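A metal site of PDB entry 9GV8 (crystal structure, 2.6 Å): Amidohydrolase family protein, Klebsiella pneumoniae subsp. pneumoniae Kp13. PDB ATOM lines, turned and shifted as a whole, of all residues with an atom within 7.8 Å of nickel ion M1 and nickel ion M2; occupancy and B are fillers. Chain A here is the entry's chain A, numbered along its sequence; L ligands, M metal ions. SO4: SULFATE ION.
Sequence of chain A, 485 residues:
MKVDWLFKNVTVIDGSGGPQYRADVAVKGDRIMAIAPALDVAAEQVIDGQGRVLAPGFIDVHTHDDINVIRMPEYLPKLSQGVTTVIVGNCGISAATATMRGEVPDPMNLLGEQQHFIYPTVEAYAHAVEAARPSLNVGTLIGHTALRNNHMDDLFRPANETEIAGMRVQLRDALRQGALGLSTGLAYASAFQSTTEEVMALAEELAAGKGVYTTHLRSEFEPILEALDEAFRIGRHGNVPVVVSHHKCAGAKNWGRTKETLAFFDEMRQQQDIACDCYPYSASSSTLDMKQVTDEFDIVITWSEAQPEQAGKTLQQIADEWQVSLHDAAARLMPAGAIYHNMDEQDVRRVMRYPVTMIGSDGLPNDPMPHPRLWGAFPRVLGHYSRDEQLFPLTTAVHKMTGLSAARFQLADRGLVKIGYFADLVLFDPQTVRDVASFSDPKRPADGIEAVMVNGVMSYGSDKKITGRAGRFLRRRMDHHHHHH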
ATOM      1  N   HIS A  62      30.360  12.076  -0.498  1.00  0.00           N
ATOM      2  CA  HIS A  62      29.721  13.306  -0.973  1.00  0.00           C
ATOM      3  C   HIS A  62      29.394  13.137  -2.456  1.00  0.00           C
ATOM      4  O   HIS A  62      30.245  13.376  -3.321  1.00  0.00           O
ATOM      5  CB  HIS A  62      30.610  14.517  -0.739  1.00  0.00           C
ATOM      6  CG  HIS A  62      29.900  15.827  -0.868  1.00  0.00           C
ATOM      7  ND1 HIS A  62      29.529  16.591   0.218  1.00  0.00           N
ATOM      8  CD2 HIS A  62      29.461  16.495  -1.955  1.00  0.00           C
ATOM      9  CE1 HIS A  62      28.911  17.680  -0.195  1.00  0.00           C
ATOM     10  NE2 HIS A  62      28.855  17.651  -1.510  1.00  0.00           N
ATOM     11  N   THR A  63      28.166  12.720  -2.749  1.00  0.00           N
ATOM     12  CA  THR A  63      27.678  12.568  -4.113  1.00  0.00           C
ATOM     13  C   THR A  63      26.340  13.290  -4.257  1.00  0.00           C
ATOM     14  O   THR A  63      25.688  13.653  -3.272  1.00  0.00           O
ATOM     15  CB  THR A  63      27.511  11.096  -4.509  1.00  0.00           C
ATOM     16  OG1 THR A  63      26.402  10.534  -3.792  1.00  0.00           O
ATOM     17  CG2 THR A  63      28.756  10.313  -4.182  1.00  0.00           C
ATOM     18  N   HIS A  64      25.948  13.490  -5.508  1.00  0.00           N
ATOM     19  CA  HIS A  64      24.612  13.955  -5.868  1.00  0.00           C
ATOM     20  C   HIS A  64      23.958  12.966  -6.826  1.00  0.00           C
ATOM     21  O   HIS A  64      23.255  13.335  -7.771  1.00  0.00           O
ATOM     22  CB  HIS A  64      24.660  15.357  -6.474  1.00  0.00           C
ATOM     23  CG  HIS A  64      25.091  16.415  -5.515  1.00  0.00           C
ATOM     24  ND1 HIS A  64      24.238  16.957  -4.580  1.00  0.00           N
ATOM     25  CD2 HIS A  64      26.280  17.041  -5.345  1.00  0.00           C
ATOM     26  CE1 HIS A  64      24.875  17.869  -3.867  1.00  0.00           C
ATOM     27  NE2 HIS A  64      26.121  17.943  -4.316  1.00  0.00           N
ATOM     28  N   GLY A  89      22.289  12.620  -1.379  1.00  0.00           N
ATOM     29  CA  GLY A  89      21.490  13.522  -0.577  1.00  0.00           C
ATOM     30  C   GLY A  89      22.287  14.539   0.202  1.00  0.00           C
ATOM     31  O   GLY A  89      21.949  14.835   1.361  1.00  0.00           O
ATOM     32  N   ASN A  90      23.335  15.105  -0.394  1.00  0.00           N
ATOM     33  CA  ASN A  90      24.172  16.081   0.279  1.00  0.00           C
ATOM     34  C   ASN A  90      23.723  17.508  -0.037  1.00  0.00           C
ATOM     35  O   ASN A  90      22.930  17.740  -0.953  1.00  0.00           O
ATOM     36  CB  ASN A  90      25.636  15.902  -0.118  1.00  0.00           C
ATOM     37  CG  ASN A  90      26.232  14.614   0.394  1.00  0.00           C
ATOM     38  OD1 ASN A  90      26.766  14.552   1.499  1.00  0.00           O
ATOM     39  ND2 ASN A  90      26.135  13.559  -0.412  1.00  0.00           N
ATOM     40  N   CYS A  91      24.239  18.449   0.746  1.00  0.00           N
ATOM     41  CA  CYS A  91      24.059  19.885   0.519  1.00  0.00           C
ATOM     42  C   CYS A  91      22.593  20.290   0.600  1.00  0.00           C
ATOM     43  O   CYS A  91      22.125  21.175  -0.122  1.00  0.00           O
ATOM     44  CB  CYS A  91      24.662  20.302  -0.823  1.00  0.00           C
ATOM     45  SG  CYS A  91      26.402  19.836  -0.993  1.00  0.00           S
ATOM     46  N   GLY A  92      21.849  19.635   1.491  1.00  0.00           N
ATOM     47  CA  GLY A  92      20.464  19.977   1.725  1.00  0.00           C
ATOM     48  C   GLY A  92      19.499  19.553   0.650  1.00  0.00           C
ATOM     49  O   GLY A  92      18.288  19.774   0.809  1.00  0.00           O
ATOM     50  N   ILE A  93      19.971  18.937  -0.435  1.00  0.00           N
ATOM     51  CA  ILE A  93      19.114  18.480  -1.516  1.00  0.00           C
ATOM     52  C   ILE A  93      19.166  16.962  -1.561  1.00  0.00           C
ATOM     53  O   ILE A  93      20.259  16.364  -1.510  1.00  0.00           O
ATOM     54  CB  ILE A  93      19.539  19.087  -2.859  1.00  0.00           C
ATOM     55  CG1 ILE A  93      21.039  18.893  -3.090  1.00  0.00           C
ATOM     56  CG2 ILE A  93      19.206  20.573  -2.904  1.00  0.00           C
ATOM     57  CD1 ILE A  93      21.499  19.267  -4.479  1.00  0.00           C
ATOM     58  N   PRO A 107      19.015  24.363  -4.995  1.00  0.00           N
ATOM     59  CA  PRO A 107      19.623  23.653  -6.119  1.00  0.00           C
ATOM     60  C   PRO A 107      19.122  22.221  -6.302  1.00  0.00           C
ATOM     61  O   PRO A 107      19.890  21.361  -6.707  1.00  0.00           O
ATOM     62  CB  PRO A 107      21.102  23.664  -5.745  1.00  0.00           C
ATOM     63  CG  PRO A 107      21.065  23.471  -4.244  1.00  0.00           C
ATOM     64  CD  PRO A 107      19.813  24.174  -3.766  1.00  0.00           C
ATOM     65  N   LEU A 110      19.737  20.040  -9.580  1.00  0.00           N
ATOM     66  CA  LEU A 110      20.933  19.272  -9.895  1.00  0.00           C
ATOM     67  C   LEU A 110      20.636  17.777  -9.937  1.00  0.00           C
ATOM     68  O   LEU A 110      21.268  17.041 -10.704  1.00  0.00           O
ATOM     69  CB  LEU A 110      22.029  19.549  -8.864  1.00  0.00           C
ATOM     70  CG  LEU A 110      22.530  20.989  -8.687  1.00  0.00           C
ATOM     71  CD1 LEU A 110      23.649  21.046  -7.651  1.00  0.00           C
ATOM     72  CD2 LEU A 110      22.995  21.590 -10.003  1.00  0.00           C
ATOM     73  N   THR A 184      22.656  19.884   4.919  1.00  0.00           N
ATOM     74  CA  THR A 184      22.190  21.252   4.742  1.00  0.00           C
ATOM     75  C   THR A 184      23.026  21.953   3.679  1.00  0.00           C
ATOM     76  O   THR A 184      24.218  21.670   3.519  1.00  0.00           O
ATOM     77  CB  THR A 184      22.244  22.056   6.053  1.00  0.00           C
ATOM     78  OG1 THR A 184      23.584  22.048   6.564  1.00  0.00           O
ATOM     79  CG2 THR A 184      21.300  21.461   7.087  1.00  0.00           C
ATOM     80  N   GLY A 185      22.380  22.859   2.964  1.00  0.00           N
ATOM     81  CA  GLY A 185      23.054  23.744   2.028  1.00  0.00           C
ATOM     82  C   GLY A 185      22.652  25.176   2.297  1.00  0.00           C
ATOM     83  O   GLY A 185      21.820  25.740   1.581  1.00  0.00           O
ATOM     84  N   LEU A 186      23.237  25.768   3.334  1.00  0.00           N
ATOM     85  CA  LEU A 186      22.734  27.044   3.845  1.00  0.00           C
ATOM     86  C   LEU A 186      23.056  28.201   2.914  1.00  0.00           C
ATOM     87  O   LEU A 186      22.326  29.206   2.910  1.00  0.00           O
ATOM     88  CB  LEU A 186      23.293  27.302   5.238  1.00  0.00           C
ATOM     89  CG  LEU A 186      23.023  26.201   6.266  1.00  0.00           C
ATOM     90  CD1 LEU A 186      23.867  26.427   7.506  1.00  0.00           C
ATOM     91  CD2 LEU A 186      21.544  26.149   6.618  1.00  0.00           C
ATOM     92  N   ALA A 187      24.132  28.103   2.139  1.00  0.00           N
ATOM     93  CA  ALA A 187      24.511  29.198   1.243  1.00  0.00           C
ATOM     94  C   ALA A 187      23.493  29.434   0.138  1.00  0.00           C
ATOM     95  O   ALA A 187      23.474  30.519  -0.447  1.00  0.00           O
ATOM     96  CB  ALA A 187      25.892  28.927   0.631  1.00  0.00           C
ATOM     97  N   TYR A 188      22.643  28.452  -0.153  1.00  0.00           N
ATOM     98  CA  TYR A 188      21.646  28.604  -1.204  1.00  0.00           C
ATOM     99  C   TYR A 188      20.452  29.395  -0.703  1.00  0.00           C
ATOM    100  O   TYR A 188      20.103  29.369   0.489  1.00  0.00           O
ATOM    101  CB  TYR A 188      21.208  27.230  -1.713  1.00  0.00           C
ATOM    102  CG  TYR A 188      22.342  26.458  -2.358  1.00  0.00           C
ATOM    103  CD1 TYR A 188      22.662  26.665  -3.694  1.00  0.00           C
ATOM    104  CD2 TYR A 188      23.095  25.552  -1.639  1.00  0.00           C
ATOM    105  CE1 TYR A 188      23.689  25.980  -4.292  1.00  0.00           C
ATOM    106  CE2 TYR A 188      24.130  24.855  -2.236  1.00  0.00           C
ATOM    107  CZ  TYR A 188      24.420  25.068  -3.564  1.00  0.00           C
ATOM    108  OH  TYR A 188      25.454  24.388  -4.156  1.00  0.00           O
ATOM    109  N   THR A 215      27.101  19.377   6.505  1.00  0.00           N
ATOM    110  CA  THR A 215      26.694  20.758   6.229  1.00  0.00           C
ATOM    111  C   THR A 215      27.512  21.351   5.101  1.00  0.00           C
ATOM    112  O   THR A 215      28.753  21.331   5.134  1.00  0.00           O
ATOM    113  CB  THR A 215      26.822  21.630   7.481  1.00  0.00           C
ATOM    114  OG1 THR A 215      26.678  23.011   7.113  1.00  0.00           O
ATOM    115  CG2 THR A 215      28.167  21.428   8.170  1.00  0.00           C
ATOM    116  N   HIS A 216      26.815  21.871   4.091  1.00  0.00           N
ATOM    117  CA  HIS A 216      27.367  22.883   3.207  1.00  0.00           C
ATOM    118  C   HIS A 216      27.273  24.207   3.952  1.00  0.00           C
ATOM    119  O   HIS A 216      26.165  24.707   4.191  1.00  0.00           O
ATOM    120  CB  HIS A 216      26.605  22.904   1.884  1.00  0.00           C
ATOM    121  CG  HIS A 216      27.102  23.916   0.896  1.00  0.00           C
ATOM    122  ND1 HIS A 216      27.171  23.663  -0.451  1.00  0.00           N
ATOM    123  CD2 HIS A 216      27.540  25.199   1.058  1.00  0.00           C
ATOM    124  CE1 HIS A 216      27.640  24.725  -1.084  1.00  0.00           C
ATOM    125  NE2 HIS A 216      27.869  25.668  -0.188  1.00  0.00           N
ATOM    126  N   LEU A 217      28.418  24.761   4.327  1.00  0.00           N
ATOM    127  CA  LEU A 217      28.445  25.921   5.225  1.00  0.00           C
ATOM    128  C   LEU A 217      27.670  27.090   4.628  1.00  0.00           C
ATOM    129  O   LEU A 217      27.520  27.211   3.412  1.00  0.00           O
ATOM    130  CB  LEU A 217      29.887  26.330   5.514  1.00  0.00           C
ATOM    131  CG  LEU A 217      30.727  25.342   6.329  1.00  0.00           C
ATOM    132  CD1 LEU A 217      32.162  25.825   6.431  1.00  0.00           C
ATOM    133  CD2 LEU A 217      30.133  25.150   7.709  1.00  0.00           C
ATOM    134  N   GLU A 220      31.430  29.852   2.455  1.00  0.00           N
ATOM    135  CA  GLU A 220      32.766  29.277   2.324  1.00  0.00           C
ATOM    136  C   GLU A 220      33.770  30.309   1.840  1.00  0.00           C
ATOM    137  O   GLU A 220      34.665  30.004   1.045  1.00  0.00           O
ATOM    138  CB  GLU A 220      32.744  28.067   1.393  1.00  0.00           C
ATOM    139  CG  GLU A 220      32.100  26.827   1.994  1.00  0.00           C
ATOM    140  CD  GLU A 220      32.588  25.556   1.336  1.00  0.00           C
ATOM    141  OE1 GLU A 220      32.371  25.392   0.119  1.00  0.00           O
ATOM    142  OE2 GLU A 220      33.183  24.716   2.040  1.00  0.00           O
ATOM    143  N   SER A 245      31.019  19.587   4.826  1.00  0.00           N
ATOM    144  CA  SER A 245      31.086  19.121   3.441  1.00  0.00           C
ATOM    145  C   SER A 245      32.000  20.013   2.609  1.00  0.00           C
ATOM    146  O   SER A 245      32.094  21.226   2.833  1.00  0.00           O
ATOM    147  CB  SER A 245      29.687  19.101   2.820  1.00  0.00           C
ATOM    148  OG  SER A 245      28.846  18.185   3.486  1.00  0.00           O
ATOM    149  N   HIS A 246      32.656  19.393   1.610  1.00  0.00           N
ATOM    150  CA  HIS A 246      33.644  19.992   0.719  1.00  0.00           C
ATOM    151  C   HIS A 246      34.337  21.206   1.305  1.00  0.00           C
ATOM    152  O   HIS A 246      34.213  22.320   0.775  1.00  0.00           O
ATOM    153  CB  HIS A 246      32.999  20.353  -0.627  1.00  0.00           C
ATOM    154  CG  HIS A 246      31.713  21.102  -0.494  1.00  0.00           C
ATOM    155  ND1 HIS A 246      31.571  22.185   0.343  1.00  0.00           N
ATOM    156  CD2 HIS A 246      30.510  20.922  -1.089  1.00  0.00           C
ATOM    157  CE1 HIS A 246      30.331  22.638   0.258  1.00  0.00           C
ATOM    158  NE2 HIS A 246      29.666  21.899  -0.611  1.00  0.00           N
ATOM    159  N   LYS A 248      36.666  24.045   1.939  1.00  0.00           N
ATOM    160  CA  LYS A 248      37.550  24.764   1.037  1.00  0.00           C
ATOM    161  C   LYS A 248      37.608  26.220   1.475  1.00  0.00           C
ATOM    162  O   LYS A 248      36.696  26.730   2.127  1.00  0.00           O
ATOM    163  CB  LYS A 248      37.062  24.655  -0.421  1.00  0.00           C
ATOM    164  CG  LYS A 248      35.798  25.446  -0.704  1.00  0.00           C
ATOM    165  CD  LYS A 248      35.189  25.101  -2.049  1.00  0.00           C
ATOM    166  CE  LYS A 248      34.629  23.686  -2.058  1.00  0.00           C
ATOM    167  NZ  LYS A 248      33.736  23.444  -3.221  1.00  0.00           N
ATOM    168  N   ASP A 277      35.020  16.460   4.666  1.00  0.00           N
ATOM    169  CA  ASP A 277      35.449  15.822   3.433  1.00  0.00           C
ATOM    170  C   ASP A 277      35.845  16.904   2.434  1.00  0.00           C
ATOM    171  O   ASP A 277      35.572  18.094   2.631  1.00  0.00           O
ATOM    172  CB  ASP A 277      34.361  14.912   2.841  1.00  0.00           C
ATOM    173  CG  ASP A 277      33.124  15.678   2.421  1.00  0.00           C
ATOM    174  OD1 ASP A 277      32.205  15.819   3.245  1.00  0.00           O
ATOM    175  OD2 ASP A 277      33.089  16.159   1.264  1.00  0.00           O
ATOM    176  N   SER A 361      34.157  12.854  -3.830  1.00  0.00           N
ATOM    177  CA  SER A 361      34.341  13.325  -5.200  1.00  0.00           C
ATOM    178  C   SER A 361      33.540  14.592  -5.475  1.00  0.00           C
ATOM    179  O   SER A 361      34.042  15.525  -6.097  1.00  0.00           O
ATOM    180  CB  SER A 361      33.957  12.226  -6.194  1.00  0.00           C
ATOM    181  OG  SER A 361      32.565  11.972  -6.168  1.00  0.00           O
ATOM    182  N   ASP A 362      32.294  14.637  -4.999  1.00  0.00           N
ATOM    183  CA  ASP A 362      31.362  15.719  -5.313  1.00  0.00           C
ATOM    184  C   ASP A 362      31.244  15.873  -6.822  1.00  0.00           C
ATOM    185  O   ASP A 362      31.329  16.975  -7.380  1.00  0.00           O
ATOM    186  CB  ASP A 362      31.781  17.026  -4.643  1.00  0.00           C
ATOM    187  CG  ASP A 362      30.690  18.086  -4.687  1.00  0.00           C
ATOM    188  OD1 ASP A 362      29.582  17.781  -5.179  1.00  0.00           O
ATOM    189  OD2 ASP A 362      30.952  19.219  -4.244  1.00  0.00           O
ATOM    190  N   GLY A 363      31.053  14.743  -7.497  1.00  0.00           N
ATOM    191  CA  GLY A 363      30.935  14.751  -8.935  1.00  0.00           C
ATOM    192  C   GLY A 363      29.534  15.118  -9.398  1.00  0.00           C
ATOM    193  O   GLY A 363      28.542  14.824  -8.749  1.00  0.00           O
ATOM    194  N   LEU A 364      29.478  15.778 -10.549  1.00  0.00           N
ATOM    195  CA  LEU A 364      28.233  16.251 -11.133  1.00  0.00           C
ATOM    196  C   LEU A 364      27.962  15.463 -12.412  1.00  0.00           C
ATOM    197  O   LEU A 364      28.471  15.833 -13.483  1.00  0.00           O
ATOM    198  CB  LEU A 364      28.290  17.748 -11.420  1.00  0.00           C
ATOM    199  CG  LEU A 364      28.166  18.804 -10.298  1.00  0.00           C
ATOM    200  CD1 LEU A 364      26.767  18.805  -9.684  1.00  0.00           C
ATOM    201  CD2 LEU A 364      29.233  18.647  -9.218  1.00  0.00           C
ATOM    202  N   ARG A 373      36.806  15.347 -11.390  1.00  0.00           N
ATOM    203  CA  ARG A 373      36.636  14.618 -10.138  1.00  0.00           C
ATOM    204  C   ARG A 373      35.590  13.517 -10.260  1.00  0.00           C
ATOM    205  O   ARG A 373      35.612  12.567  -9.456  1.00  0.00           O
ATOM    206  CB  ARG A 373      36.254  15.578  -9.020  1.00  0.00           C
ATOM    207  CG  ARG A 373      34.907  16.258  -9.205  1.00  0.00           C
ATOM    208  CD  ARG A 373      34.837  17.536  -8.388  1.00  0.00           C
ATOM    209  NE  ARG A 373      33.545  18.202  -8.538  1.00  0.00           N
ATOM    210  CZ  ARG A 373      33.302  19.442  -8.136  1.00  0.00           C
ATOM    211  NH1 ARG A 373      34.236  20.178  -7.567  1.00  0.00           N
ATOM    212  NH2 ARG A 373      32.088  19.947  -8.301  1.00  0.00           N
HETATM  213  S   SO4 L   1      27.500  21.691  -4.506  1.00  0.00           S
HETATM  214  O1  SO4 L   1      28.056  22.392  -5.699  1.00  0.00           O
HETATM  215  O2  SO4 L   1      26.017  21.562  -4.635  1.00  0.00           O
HETATM  216  O3  SO4 L   1      28.121  20.332  -4.396  1.00  0.00           O
HETATM  217  O4  SO4 L   1      27.824  22.477  -3.263  1.00  0.00           O
HETATM  218 NI    NI M   1      27.723  21.850  -1.409  1.00  0.00          NI
HETATM  219 NI    NI M   2      27.504  18.678  -2.900  1.00  0.00          NI
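Nickel ion M1 is bound by an oxygen (O4) of the ligand (2.0 Å), a ring nitrogen (NE2) of His 246 (2.1 Å), a ring nitrogen (ND1) of His 216 (2.1 Å) and the side-chain sulfur (SG) of Cys 91 (2.4 Å).
Nickel ion M2 is bound by NE2 of His 64 (2.1 Å), NE2 of His 62 (2.2 Å), O3 of the ligand (2.3 Å) and SG of Cys 91 (2.5 Å). Nickel ion M2 has four donor atoms within binding distance.
ND1 of His 246 lies within hydrogen-bond range of OE1 of Glu 220 (3.3 Å). OD2 of Asp 277 lies within hydrogen-bond range of N of His 246 (3.3 Å). The backbone NH (N) of His 216 is in hydrogen-bond range of the backbone carbonyl oxygen (O) of Thr 184 (2.7 Å). N of Leu 186 is in hydrogen-bond range of O of His 216, at 3.2 Å. The backbone carbonyl oxygen (O) of His 62 is in hydrogen-bond range of the backbone NH (N) of Asp 362. The guanidinium group of Arg 373 is in hydrogen-bond range of the backbone carbonyl oxygen of Asp 362.
Of the 28 residues printed, 3 come within 4 Å of nickel ion M1.
Merely in contact with nickel ion M2: Asp 362 (3.2 Å). Four residues have an atom within 4 Å of nickel ion M2: His 62, His 64, Cys 91 and Asp 362. The nearest printed residue that does not touch nickel ion M2 is His 246 (4.2 Å).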
